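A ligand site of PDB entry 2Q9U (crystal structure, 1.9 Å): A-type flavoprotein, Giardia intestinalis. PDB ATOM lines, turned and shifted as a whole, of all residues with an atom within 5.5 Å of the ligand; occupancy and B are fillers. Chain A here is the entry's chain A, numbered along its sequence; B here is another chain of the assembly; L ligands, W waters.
An oxygen (O8) of the ligand sits at hydrogen-bond distance from the backbone NH (N) of Tyr 267, 2.6 Å away. An oxygen (O8) of the ligand sits at hydrogen-bond distance from the backbone NH of Met 266 (2.6 Å). The backbone NH (N) of Thr 270 is in hydrogen-bond range of an oxygen (O7) of the ligand. OG1 of Thr 270 is in hydrogen-bond range of O7 of the ligand (2.7 Å). The side-chain hydroxyl (OG) of Ser 265 sits at hydrogen-bond distance from an oxygen (O7) of the ligand (2.7 Å). N of Ser 353 is in hydrogen-bond range of O1 of the ligand (2.8 Å). The backbone NH of Asn 320 is in hydrogen-bond range of an oxygen (O2) of the ligand (2.8 Å). O of Thr 317 is in hydrogen-bond range of O3 of the ligand. The backbone NH (N) of Trp 352 sits at hydrogen-bond distance from an oxygen (O1) of the ligand. N of Thr 269 sits at hydrogen-bond distance from O9 of the ligand. An oxygen (O9) of the ligand sits at hydrogen-bond distance from the side-chain hydroxyl (OG1) of Thr 269, at 2.9 Å. O2 of the ligand lies within hydrogen-bond range of N of Asn 319, at 3.0 Å. O9 of the ligand sits at hydrogen-bond distance from N of Gly 268 (3.1 Å). O of Phe 382 sits at hydrogen-bond distance from O5 of the ligand (3.1 Å). N1 of the ligand is in hydrogen-bond range of N of Gly 351 (3.2 Å).
Water W1 bridges O2 of the ligand (2.7 Å) and NE1 of Trp 352 (3.2 Å). Water W4 lies within hydrogen-bond range of the side-chain amide oxygen (OD1) of Asn 320 (2.6 Å), a nitrogen (N2) of the ligand (2.7 Å) and the backbone carbonyl oxygen (O) of Ser 353 (2.9 Å). Water W6 bridges the side-chain amide oxygen (OD1) of Asn 319 (2.8 Å) and a nitrogen (N3) of the ligand (2.9 Å). Water W5 bridges the backbone carbonyl oxygen of Phe 382 (2.9 Å) and an oxygen (O9) of the ligand (3.0 Å).
The side-chain hydroxyl (OH) of Tyr 267 sits at hydrogen-bond distance from the side-chain carboxylate (OE2) of Glu 87 of chain B. The backbone NH of Ala 349 sits at hydrogen-bond distance from the side-chain hydroxyl of Thr 270 (3.2 Å). The side-chain hydroxyl of Ser 265 is in hydrogen-bond range of the backbone NH of Gly 268. N of Thr 317 sits at hydrogen-bond distance from O of Ala 349 (3.2 Å). The backbone carbonyl oxygen of Phe 382 sits at hydrogen-bond distance from the side-chain hydroxyl of Thr 269, at 3.4 Å. The backbone carbonyl oxygen of Phe 350 is in hydrogen-bond range of the backbone NH of Phe 382 (2.8 Å).
Residues that only touch the ligand: Pro 316 (3.3 Å), Leu 318 (3.3 Å), Ala 349 (3.4 Å), Trp 153 of chain B (3.4 Å), Glu 87 of chain B (3.5 Å), Phe 350 (3.5 Å) and His 31 of chain B (3.95 Å). Hydrophobic or aromatic side chains that line the ligand: Met 266, Tyr 267, Pro 316, Leu 318, Ala 349, Phe 350, Trp 352, Phe 382, His 31 of chain B and Trp 153 of chain B. Within 4 Å of the ligand: Ser 265, Met 266, Tyr 267, Gly 268, Thr 269, Thr 270, Pro 316, Thr 317, Leu 318, Asn 319, Asn 320, Ala 349, Phe 350, Gly 351, Trp 352, Ser 353, Phe 382, His 31 of chain B, Glu 87 of chain B and Trp 153 of chain B. The nearest printed residue that does not touch the ligand is His 152 of chain B (4.1 Å).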
ATOM      1  N   ASP A 264     -12.559  21.219  21.415  1.00  0.00           N
ATOM      2  CA  ASP A 264     -12.746  20.526  22.677  1.00  0.00           C
ATOM      3  C   ASP A 264     -11.401  19.849  22.957  1.00  0.00           C
ATOM      4  O   ASP A 264     -10.550  19.723  22.083  1.00  0.00           O
ATOM      5  CB  ASP A 264     -13.891  19.515  22.572  1.00  0.00           C
ATOM      6  CG  ASP A 264     -14.502  19.155  23.931  1.00  0.00           C
ATOM      7  OD1 ASP A 264     -13.847  19.411  24.982  1.00  0.00           O
ATOM      8  OD2 ASP A 264     -15.618  18.587  23.944  1.00  0.00           O
ATOM      9  N   SER A 265     -11.186  19.420  24.186  1.00  0.00           N
ATOM     10  CA  SER A 265      -9.893  18.888  24.588  1.00  0.00           C
ATOM     11  C   SER A 265     -10.182  17.951  25.766  1.00  0.00           C
ATOM     12  O   SER A 265     -11.117  18.185  26.496  1.00  0.00           O
ATOM     13  CB  SER A 265      -8.964  20.055  25.020  1.00  0.00           C
ATOM     14  OG  SER A 265      -7.639  19.606  25.316  1.00  0.00           O
ATOM     15  N   MET A 266      -9.395  16.895  25.939  1.00  0.00           N
ATOM     16  CA  MET A 266      -9.563  15.960  27.059  1.00  0.00           C
ATOM     17  C   MET A 266      -8.534  16.171  28.175  1.00  0.00           C
ATOM     18  O   MET A 266      -8.880  16.152  29.376  1.00  0.00           O
ATOM     19  CB  MET A 266      -9.490  14.532  26.519  1.00  0.00           C
ATOM     20  CG  MET A 266     -10.675  14.228  25.613  1.00  0.00           C
ATOM     21  SD  MET A 266     -10.677  12.544  25.000  1.00  0.00           S
ATOM     22  CE  MET A 266      -9.282  12.594  23.876  1.00  0.00           C
ATOM     23  N   TYR A 267      -7.265  16.334  27.806  1.00  0.00           N
ATOM     24  CA  TYR A 267      -6.198  16.592  28.796  1.00  0.00           C
ATOM     25  C   TYR A 267      -5.508  17.951  28.583  1.00  0.00           C
ATOM     26  O   TYR A 267      -4.482  18.238  29.196  1.00  0.00           O
ATOM     27  CB  TYR A 267      -5.177  15.450  28.828  1.00  0.00           C
ATOM     28  CG  TYR A 267      -5.694  14.211  29.531  1.00  0.00           C
ATOM     29  CD1 TYR A 267      -5.554  14.067  30.938  1.00  0.00           C
ATOM     30  CD2 TYR A 267      -6.302  13.181  28.818  1.00  0.00           C
ATOM     31  CE1 TYR A 267      -6.027  12.908  31.614  1.00  0.00           C
ATOM     32  CE2 TYR A 267      -6.786  12.018  29.482  1.00  0.00           C
ATOM     33  CZ  TYR A 267      -6.646  11.900  30.879  1.00  0.00           C
ATOM     34  OH  TYR A 267      -7.124  10.771  31.533  1.00  0.00           O
ATOM     35  N   GLY A 268      -6.066  18.787  27.718  1.00  0.00           N
ATOM     36  CA  GLY A 268      -5.680  20.209  27.733  1.00  0.00           C
ATOM     37  C   GLY A 268      -4.518  20.632  26.848  1.00  0.00           C
ATOM     38  O   GLY A 268      -4.217  21.821  26.770  1.00  0.00           O
ATOM     39  N   THR A 269      -3.867  19.688  26.158  1.00  0.00           N
ATOM     40  CA  THR A 269      -2.755  20.090  25.278  1.00  0.00           C
ATOM     41  C   THR A 269      -3.238  20.783  23.991  1.00  0.00           C
ATOM     42  O   THR A 269      -2.603  21.752  23.528  1.00  0.00           O
ATOM     43  CB  THR A 269      -1.763  18.952  24.944  1.00  0.00           C
ATOM     44  OG1 THR A 269      -2.394  17.961  24.125  1.00  0.00           O
ATOM     45  CG2 THR A 269      -1.222  18.303  26.251  1.00  0.00           C
ATOM     46  N   THR A 270      -4.347  20.303  23.423  1.00  0.00           N
ATOM     47  CA  THR A 270      -4.977  20.985  22.278  1.00  0.00           C
ATOM     48  C   THR A 270      -5.430  22.393  22.708  1.00  0.00           C
ATOM     49  O   THR A 270      -5.331  23.374  21.946  1.00  0.00           O
ATOM     50  CB  THR A 270      -6.163  20.198  21.664  1.00  0.00           C
ATOM     51  OG1 THR A 270      -5.741  18.882  21.282  1.00  0.00           O
ATOM     52  CG2 THR A 270      -6.673  20.907  20.398  1.00  0.00           C
ATOM     53  N   HIS A 271      -5.950  22.487  23.935  1.00  0.00           N
ATOM     54  CA  HIS A 271      -6.275  23.790  24.542  1.00  0.00           C
ATOM     55  C   HIS A 271      -5.078  24.751  24.655  1.00  0.00           C
ATOM     56  O   HIS A 271      -5.192  25.934  24.291  1.00  0.00           O
ATOM     57  CB  HIS A 271      -6.915  23.598  25.912  1.00  0.00           C
ATOM     58  CG  HIS A 271      -7.286  24.893  26.564  1.00  0.00           C
ATOM     59  ND1 HIS A 271      -8.496  25.503  26.351  1.00  0.00           N
ATOM     60  CD2 HIS A 271      -6.575  25.724  27.370  1.00  0.00           C
ATOM     61  CE1 HIS A 271      -8.532  26.647  27.018  1.00  0.00           C
ATOM     62  NE2 HIS A 271      -7.378  26.799  27.654  1.00  0.00           N
ATOM     63  N   PRO A 316      -8.608  16.775  19.842  1.00  0.00           N
ATOM     64  CA  PRO A 316      -7.801  15.542  19.819  1.00  0.00           C
ATOM     65  C   PRO A 316      -8.531  14.418  19.097  1.00  0.00           C
ATOM     66  O   PRO A 316      -9.758  14.476  18.882  1.00  0.00           O
ATOM     67  CB  PRO A 316      -7.622  15.202  21.312  1.00  0.00           C
ATOM     68  CG  PRO A 316      -8.765  15.825  22.000  1.00  0.00           C
ATOM     69  CD  PRO A 316      -9.019  17.128  21.214  1.00  0.00           C
ATOM     70  N   THR A 317      -7.769  13.398  18.687  1.00  0.00           N
ATOM     71  CA  THR A 317      -8.364  12.204  18.130  1.00  0.00           C
ATOM     72  C   THR A 317      -8.994  11.395  19.267  1.00  0.00           C
ATOM     73  O   THR A 317      -8.334  11.057  20.261  1.00  0.00           O
ATOM     74  CB  THR A 317      -7.350  11.371  17.308  1.00  0.00           C
ATOM     75  OG1 THR A 317      -6.949  12.120  16.145  1.00  0.00           O
ATOM     76  CG2 THR A 317      -7.989  10.060  16.823  1.00  0.00           C
ATOM     77  N   LEU A 318     -10.289  11.136  19.132  1.00  0.00           N
ATOM     78  CA  LEU A 318     -11.000  10.272  20.061  1.00  0.00           C
ATOM     79  C   LEU A 318     -11.615   9.141  19.250  1.00  0.00           C
ATOM     80  O   LEU A 318     -12.464   9.407  18.375  1.00  0.00           O
ATOM     81  CB  LEU A 318     -12.085  11.066  20.792  1.00  0.00           C
ATOM     82  CG  LEU A 318     -12.963  10.303  21.819  1.00  0.00           C
ATOM     83  CD1 LEU A 318     -12.134   9.650  22.940  1.00  0.00           C
ATOM     84  CD2 LEU A 318     -14.037  11.253  22.414  1.00  0.00           C
ATOM     85  N   ASN A 319     -11.152   7.917  19.497  1.00  0.00           N
ATOM     86  CA  ASN A 319     -11.678   6.716  18.829  1.00  0.00           C
ATOM     87  C   ASN A 319     -11.713   6.889  17.331  1.00  0.00           C
ATOM     88  O   ASN A 319     -12.757   6.701  16.702  1.00  0.00           O
ATOM     89  CB  ASN A 319     -13.079   6.361  19.361  1.00  0.00           C
ATOM     90  CG  ASN A 319     -13.111   6.213  20.889  1.00  0.00           C
ATOM     91  OD1 ASN A 319     -12.167   5.701  21.480  1.00  0.00           O
ATOM     92  ND2 ASN A 319     -14.179   6.688  21.516  1.00  0.00           N
ATOM     93  N   ASN A 320     -10.565   7.288  16.776  1.00  0.00           N
ATOM     94  CA  ASN A 320     -10.335   7.380  15.326  1.00  0.00           C
ATOM     95  C   ASN A 320     -11.099   8.484  14.612  1.00  0.00           C
ATOM     96  O   ASN A 320     -11.203   8.474  13.386  1.00  0.00           O
ATOM     97  CB  ASN A 320     -10.621   6.029  14.639  1.00  0.00           C
ATOM     98  CG  ASN A 320      -9.742   4.908  15.171  1.00  0.00           C
ATOM     99  OD1 ASN A 320      -8.512   5.036  15.183  1.00  0.00           O
ATOM    100  ND2 ASN A 320     -10.360   3.810  15.628  1.00  0.00           N
ATOM    101  N   THR A 321     -11.615   9.444  15.374  1.00  0.00           N
ATOM    102  CA  THR A 321     -12.266  10.589  14.760  1.00  0.00           C
ATOM    103  C   THR A 321     -12.142  11.837  15.648  1.00  0.00           C
ATOM    104  O   THR A 321     -11.341  11.858  16.577  1.00  0.00           O
ATOM    105  CB  THR A 321     -13.731  10.256  14.337  1.00  0.00           C
ATOM    106  OG1 THR A 321     -14.281  11.362  13.609  1.00  0.00           O
ATOM    107  CG2 THR A 321     -14.629   9.891  15.549  1.00  0.00           C
ATOM    108  N   ALA A 349      -4.158  17.362  18.913  1.00  0.00           N
ATOM    109  CA  ALA A 349      -3.284  16.281  19.387  1.00  0.00           C
ATOM    110  C   ALA A 349      -3.758  14.911  18.931  1.00  0.00           C
ATOM    111  O   ALA A 349      -4.910  14.727  18.555  1.00  0.00           O
ATOM    112  CB  ALA A 349      -3.210  16.337  20.926  1.00  0.00           C
ATOM    113  N   PHE A 350      -2.861  13.928  18.943  1.00  0.00           N
ATOM    114  CA  PHE A 350      -3.277  12.534  18.791  1.00  0.00           C
ATOM    115  C   PHE A 350      -2.290  11.667  19.567  1.00  0.00           C
ATOM    116  O   PHE A 350      -1.218  12.139  19.977  1.00  0.00           O
ATOM    117  CB  PHE A 350      -3.345  12.130  17.306  1.00  0.00           C
ATOM    118  CG  PHE A 350      -2.005  12.164  16.597  1.00  0.00           C
ATOM    119  CD1 PHE A 350      -1.537  13.338  16.033  1.00  0.00           C
ATOM    120  CD2 PHE A 350      -1.214  11.009  16.522  1.00  0.00           C
ATOM    121  CE1 PHE A 350      -0.279  13.372  15.368  1.00  0.00           C
ATOM    122  CE2 PHE A 350       0.034  11.026  15.871  1.00  0.00           C
ATOM    123  CZ  PHE A 350       0.502  12.214  15.303  1.00  0.00           C
ATOM    124  N   GLY A 351      -2.674  10.417  19.776  1.00  0.00           N
ATOM    125  CA  GLY A 351      -1.880   9.469  20.532  1.00  0.00           C
ATOM    126  C   GLY A 351      -1.095   8.543  19.630  1.00  0.00           C
ATOM    127  O   GLY A 351       0.106   8.331  19.848  1.00  0.00           O
ATOM    128  N   TRP A 352      -1.765   7.948  18.657  1.00  0.00           N
ATOM    129  CA  TRP A 352      -1.113   6.958  17.787  1.00  0.00           C
ATOM    130  C   TRP A 352      -1.473   7.087  16.331  1.00  0.00           C
ATOM    131  O   TRP A 352      -0.648   6.779  15.469  1.00  0.00           O
ATOM    132  CB  TRP A 352      -1.348   5.524  18.268  1.00  0.00           C
ATOM    133  CG  TRP A 352      -2.776   5.189  18.591  1.00  0.00           C
ATOM    134  CD1 TRP A 352      -3.677   4.582  17.782  1.00  0.00           C
ATOM    135  CD2 TRP A 352      -3.447   5.456  19.820  1.00  0.00           C
ATOM    136  NE1 TRP A 352      -4.886   4.445  18.429  1.00  0.00           N
ATOM    137  CE2 TRP A 352      -4.763   4.968  19.692  1.00  0.00           C
ATOM    138  CE3 TRP A 352      -3.065   6.059  21.034  1.00  0.00           C
ATOM    139  CZ2 TRP A 352      -5.706   5.073  20.724  1.00  0.00           C
ATOM    140  CZ3 TRP A 352      -4.005   6.161  22.057  1.00  0.00           C
ATOM    141  CH2 TRP A 352      -5.305   5.667  21.891  1.00  0.00           C
ATOM    142  N   SER A 353      -2.672   7.581  16.040  1.00  0.00           N
ATOM    143  CA  SER A 353      -3.122   7.706  14.661  1.00  0.00           C
ATOM    144  C   SER A 353      -3.908   9.013  14.502  1.00  0.00           C
ATOM    145  O   SER A 353      -4.928   9.207  15.137  1.00  0.00           O
ATOM    146  CB  SER A 353      -3.946   6.494  14.227  1.00  0.00           C
ATOM    147  OG  SER A 353      -4.501   6.671  12.913  1.00  0.00           O
ATOM    148  N   ASN A 354      -3.362   9.907  13.684  1.00  0.00           N
ATOM    149  CA  ASN A 354      -3.958  11.231  13.446  1.00  0.00           C
ATOM    150  C   ASN A 354      -5.243  11.157  12.621  1.00  0.00           C
ATOM    151  O   ASN A 354      -5.189  10.954  11.402  1.00  0.00           O
ATOM    152  CB  ASN A 354      -2.914  12.151  12.797  1.00  0.00           C
ATOM    153  CG  ASN A 354      -3.485  13.502  12.372  1.00  0.00           C
ATOM    154  OD1 ASN A 354      -4.268  14.118  13.109  1.00  0.00           O
ATOM    155  ND2 ASN A 354      -3.105  13.962  11.172  1.00  0.00           N
ATOM    156  N   LYS A 381       1.859  14.374  18.639  1.00  0.00           N
ATOM    157  CA  LYS A 381       1.614  13.241  19.525  1.00  0.00           C
ATOM    158  C   LYS A 381       1.745  13.543  21.017  1.00  0.00           C
ATOM    159  O   LYS A 381       2.783  13.875  21.498  1.00  0.00           O
ATOM    160  CB  LYS A 381       2.446  12.025  19.091  1.00  0.00           C
ATOM    161  CG  LYS A 381       2.468  10.905  20.039  1.00  0.00           C
ATOM    162  CD  LYS A 381       3.514   9.875  19.627  1.00  0.00           C
ATOM    163  CE  LYS A 381       3.415   9.522  18.204  1.00  0.00           C
ATOM    164  NZ  LYS A 381       3.446   8.055  17.992  1.00  0.00           N
ATOM    165  N   PHE A 382       0.619  13.469  21.696  1.00  0.00           N
ATOM    166  CA  PHE A 382       0.486  13.574  23.134  1.00  0.00           C
ATOM    167  C   PHE A 382       0.650  14.940  23.776  1.00  0.00           C
ATOM    168  O   PHE A 382      -0.227  15.389  24.437  1.00  0.00           O
ATOM    169  CB  PHE A 382       1.275  12.502  23.855  1.00  0.00           C
ATOM    170  CG  PHE A 382       0.596  11.198  23.878  1.00  0.00           C
ATOM    171  CD1 PHE A 382      -0.653  11.076  24.435  1.00  0.00           C
ATOM    172  CD2 PHE A 382       1.166  10.108  23.305  1.00  0.00           C
ATOM    173  CE1 PHE A 382      -1.284   9.916  24.421  1.00  0.00           C
ATOM    174  CE2 PHE A 382       0.519   8.910  23.311  1.00  0.00           C
ATOM    175  CZ  PHE A 382      -0.702   8.816  23.864  1.00  0.00           C
ATOM    176  N   ASN A 383       1.787  15.577  23.549  1.00  0.00           N
ATOM    177  CA  ASN A 383       2.105  16.800  24.233  1.00  0.00           C
ATOM    178  C   ASN A 383       2.740  17.882  23.374  1.00  0.00           C
ATOM    179  O   ASN A 383       3.329  17.580  22.397  1.00  0.00           O
ATOM    180  CB  ASN A 383       3.013  16.406  25.372  1.00  0.00           C
ATOM    181  CG  ASN A 383       3.107  17.423  26.440  1.00  0.00           C
ATOM    182  OD1 ASN A 383       2.446  18.417  26.439  1.00  0.00           O
ATOM    183  ND2 ASN A 383       3.930  17.148  27.398  1.00  0.00           N
ATOM    184  N   HIS B  31     -12.849  13.481  30.456  1.00  0.00           N
ATOM    185  CA  HIS B  31     -12.555  13.347  29.023  1.00  0.00           C
ATOM    186  C   HIS B  31     -13.843  13.179  28.208  1.00  0.00           C
ATOM    187  O   HIS B  31     -13.921  12.383  27.287  1.00  0.00           O
ATOM    188  CB  HIS B  31     -11.471  12.266  28.747  1.00  0.00           C
ATOM    189  CG  HIS B  31     -11.917  10.851  28.931  1.00  0.00           C
ATOM    190  ND1 HIS B  31     -12.919  10.263  28.177  1.00  0.00           N
ATOM    191  CD2 HIS B  31     -11.449   9.875  29.756  1.00  0.00           C
ATOM    192  CE1 HIS B  31     -13.059   8.990  28.540  1.00  0.00           C
ATOM    193  NE2 HIS B  31     -12.188   8.739  29.502  1.00  0.00           N
ATOM    194  N   GLU B  87      -1.659   7.221  30.759  1.00  0.00           N
ATOM    195  CA  GLU B  87      -2.732   8.224  30.783  1.00  0.00           C
ATOM    196  C   GLU B  87      -2.728   9.005  32.103  1.00  0.00           C
ATOM    197  O   GLU B  87      -2.426   8.450  33.179  1.00  0.00           O
ATOM    198  CB  GLU B  87      -4.108   7.595  30.481  1.00  0.00           C
ATOM    199  CG  GLU B  87      -5.156   8.653  30.048  1.00  0.00           C
ATOM    200  CD  GLU B  87      -6.491   8.041  29.751  1.00  0.00           C
ATOM    201  OE1 GLU B  87      -6.514   6.834  29.405  1.00  0.00           O
ATOM    202  OE2 GLU B  87      -7.508   8.753  29.909  1.00  0.00           O
ATOM    203  N   HIS B 152      -6.703   0.201  26.690  1.00  0.00           N
ATOM    204  CA  HIS B 152      -7.160   0.863  25.464  1.00  0.00           C
ATOM    205  C   HIS B 152      -6.091   1.741  24.781  1.00  0.00           C
ATOM    206  O   HIS B 152      -6.368   2.359  23.734  1.00  0.00           O
ATOM    207  CB  HIS B 152      -8.399   1.721  25.788  1.00  0.00           C
ATOM    208  CG  HIS B 152      -8.100   2.848  26.717  1.00  0.00           C
ATOM    209  ND1 HIS B 152      -8.042   4.165  26.286  1.00  0.00           N
ATOM    210  CD2 HIS B 152      -7.784   2.857  28.029  1.00  0.00           C
ATOM    211  CE1 HIS B 152      -7.724   4.935  27.308  1.00  0.00           C
ATOM    212  NE2 HIS B 152      -7.551   4.169  28.380  1.00  0.00           N
ATOM    213  N   TRP B 153      -4.884   1.838  25.362  1.00  0.00           N
ATOM    214  CA  TRP B 153      -3.781   2.605  24.725  1.00  0.00           C
ATOM    215  C   TRP B 153      -2.683   1.643  24.249  1.00  0.00           C
ATOM    216  O   TRP B 153      -2.621   0.495  24.739  1.00  0.00           O
ATOM    217  CB  TRP B 153      -3.228   3.647  25.713  1.00  0.00           C
ATOM    218  CG  TRP B 153      -3.927   4.979  25.675  1.00  0.00           C
ATOM    219  CD1 TRP B 153      -5.172   5.257  25.142  1.00  0.00           C
ATOM    220  CD2 TRP B 153      -3.433   6.213  26.215  1.00  0.00           C
ATOM    221  NE1 TRP B 153      -5.458   6.589  25.304  1.00  0.00           N
ATOM    222  CE2 TRP B 153      -4.422   7.203  25.960  1.00  0.00           C
ATOM    223  CE3 TRP B 153      -2.255   6.580  26.870  1.00  0.00           C
ATOM    224  CZ2 TRP B 153      -4.260   8.533  26.363  1.00  0.00           C
ATOM    225  CZ3 TRP B 153      -2.098   7.927  27.256  1.00  0.00           C
ATOM    226  CH2 TRP B 153      -3.092   8.867  27.006  1.00  0.00           C
ATOM    227  N   ILE B 203     -15.292   3.195  26.835  1.00  0.00           N
ATOM    228  CA  ILE B 203     -13.823   3.268  26.773  1.00  0.00           C
ATOM    229  C   ILE B 203     -13.273   2.151  25.877  1.00  0.00           C
ATOM    230  O   ILE B 203     -12.344   2.375  25.088  1.00  0.00           O
ATOM    231  CB  ILE B 203     -13.183   3.214  28.186  1.00  0.00           C
ATOM    232  CG1 ILE B 203     -13.839   4.269  29.119  1.00  0.00           C
ATOM    233  CG2 ILE B 203     -11.627   3.340  28.106  1.00  0.00           C
ATOM    234  CD1 ILE B 203     -13.769   5.691  28.601  1.00  0.00           C
ATOM    235  N   LEU B 206     -14.484  -0.264  20.994  1.00  0.00           N
ATOM    236  CA  LEU B 206     -13.857  -0.578  19.716  1.00  0.00           C
ATOM    237  C   LEU B 206     -12.710  -1.610  19.829  1.00  0.00           C
ATOM    238  O   LEU B 206     -12.052  -1.939  18.813  1.00  0.00           O
ATOM    239  CB  LEU B 206     -13.328   0.692  19.016  1.00  0.00           C
ATOM    240  CG  LEU B 206     -12.188   1.522  19.625  1.00  0.00           C
ATOM    241  CD1 LEU B 206     -11.670   2.506  18.607  1.00  0.00           C
ATOM    242  CD2 LEU B 206     -12.602   2.310  20.893  1.00  0.00           C
HETATM  243  N1  LIG L   1      -5.387   8.814  19.960  1.00  0.00           N
HETATM  244  C1  LIG L   1      -5.430   8.337  18.680  1.00  0.00           C
HETATM  245  O1  LIG L   1      -4.491   8.595  17.903  1.00  0.00           O
HETATM  246  N2  LIG L   1      -6.487   7.559  18.269  1.00  0.00           N
HETATM  247  C2  LIG L   1      -7.550   7.275  19.121  1.00  0.00           C
HETATM  248  O2  LIG L   1      -8.529   6.693  18.652  1.00  0.00           O
HETATM  249  C3  LIG L   1      -7.516   7.778  20.434  1.00  0.00           C
HETATM  250  N3  LIG L   1      -8.528   7.507  21.348  1.00  0.00           N
HETATM  251  C4  LIG L   1      -8.433   8.018  22.641  1.00  0.00           C
HETATM  252  C5  LIG L   1      -9.450   7.753  23.574  1.00  0.00           C
HETATM  253  C6  LIG L   1      -9.373   8.269  24.883  1.00  0.00           C
HETATM  254  C7  LIG L   1     -10.383   7.784  25.892  1.00  0.00           C
HETATM  255  C8  LIG L   1      -8.281   9.040  25.272  1.00  0.00           C
HETATM  256  C9  LIG L   1      -8.217   9.699  26.626  1.00  0.00           C
HETATM  257  C10 LIG L   1      -7.273   9.301  24.349  1.00  0.00           C
HETATM  258  C11 LIG L   1      -7.337   8.799  23.039  1.00  0.00           C
HETATM  259  N4  LIG L   1      -6.336   9.066  22.112  1.00  0.00           N
HETATM  260  C12 LIG L   1      -6.413   8.539  20.840  1.00  0.00           C
HETATM  261  C13 LIG L   1      -5.132   9.892  22.468  1.00  0.00           C
HETATM  262  C14 LIG L   1      -5.447  11.392  22.511  1.00  0.00           C
HETATM  263  O3  LIG L   1      -5.749  11.912  21.219  1.00  0.00           O
HETATM  264  C15 LIG L   1      -4.246  12.032  23.199  1.00  0.00           C
HETATM  265  O4  LIG L   1      -4.336  11.730  24.580  1.00  0.00           O
HETATM  266  C16 LIG L   1      -4.155  13.541  23.048  1.00  0.00           C
HETATM  267  O5  LIG L   1      -2.887  13.983  23.505  1.00  0.00           O
HETATM  268  C17 LIG L   1      -5.234  14.255  23.873  1.00  0.00           C
HETATM  269  O6  LIG L   1      -5.242  15.630  23.525  1.00  0.00           O
HETATM  270  P1  LIG L   1      -5.714  16.692  24.610  1.00  0.00           P
HETATM  271  O7  LIG L   1      -5.993  17.966  23.850  1.00  0.00           O
HETATM  272  O8  LIG L   1      -6.952  16.138  25.260  1.00  0.00           O
HETATM  273  O9  LIG L   1      -4.644  16.912  25.668  1.00  0.00           O
HETATM  274  O   HOH W   1      -8.062   4.037  18.636  1.00  0.00           O
HETATM  275  O   HOH W   2      -8.166   4.577  23.416  1.00  0.00           O
HETATM  276  O   HOH W   3      -2.663  12.460  26.775  1.00  0.00           O
HETATM  277  O   HOH W   4      -6.709   6.923  15.632  1.00  0.00           O
HETATM  278  O   HOH W   5      -2.333  15.224  26.475  1.00  0.00           O
HETATM  279  O   HOH W   6      -9.535   4.760  21.031  1.00  0.00           O
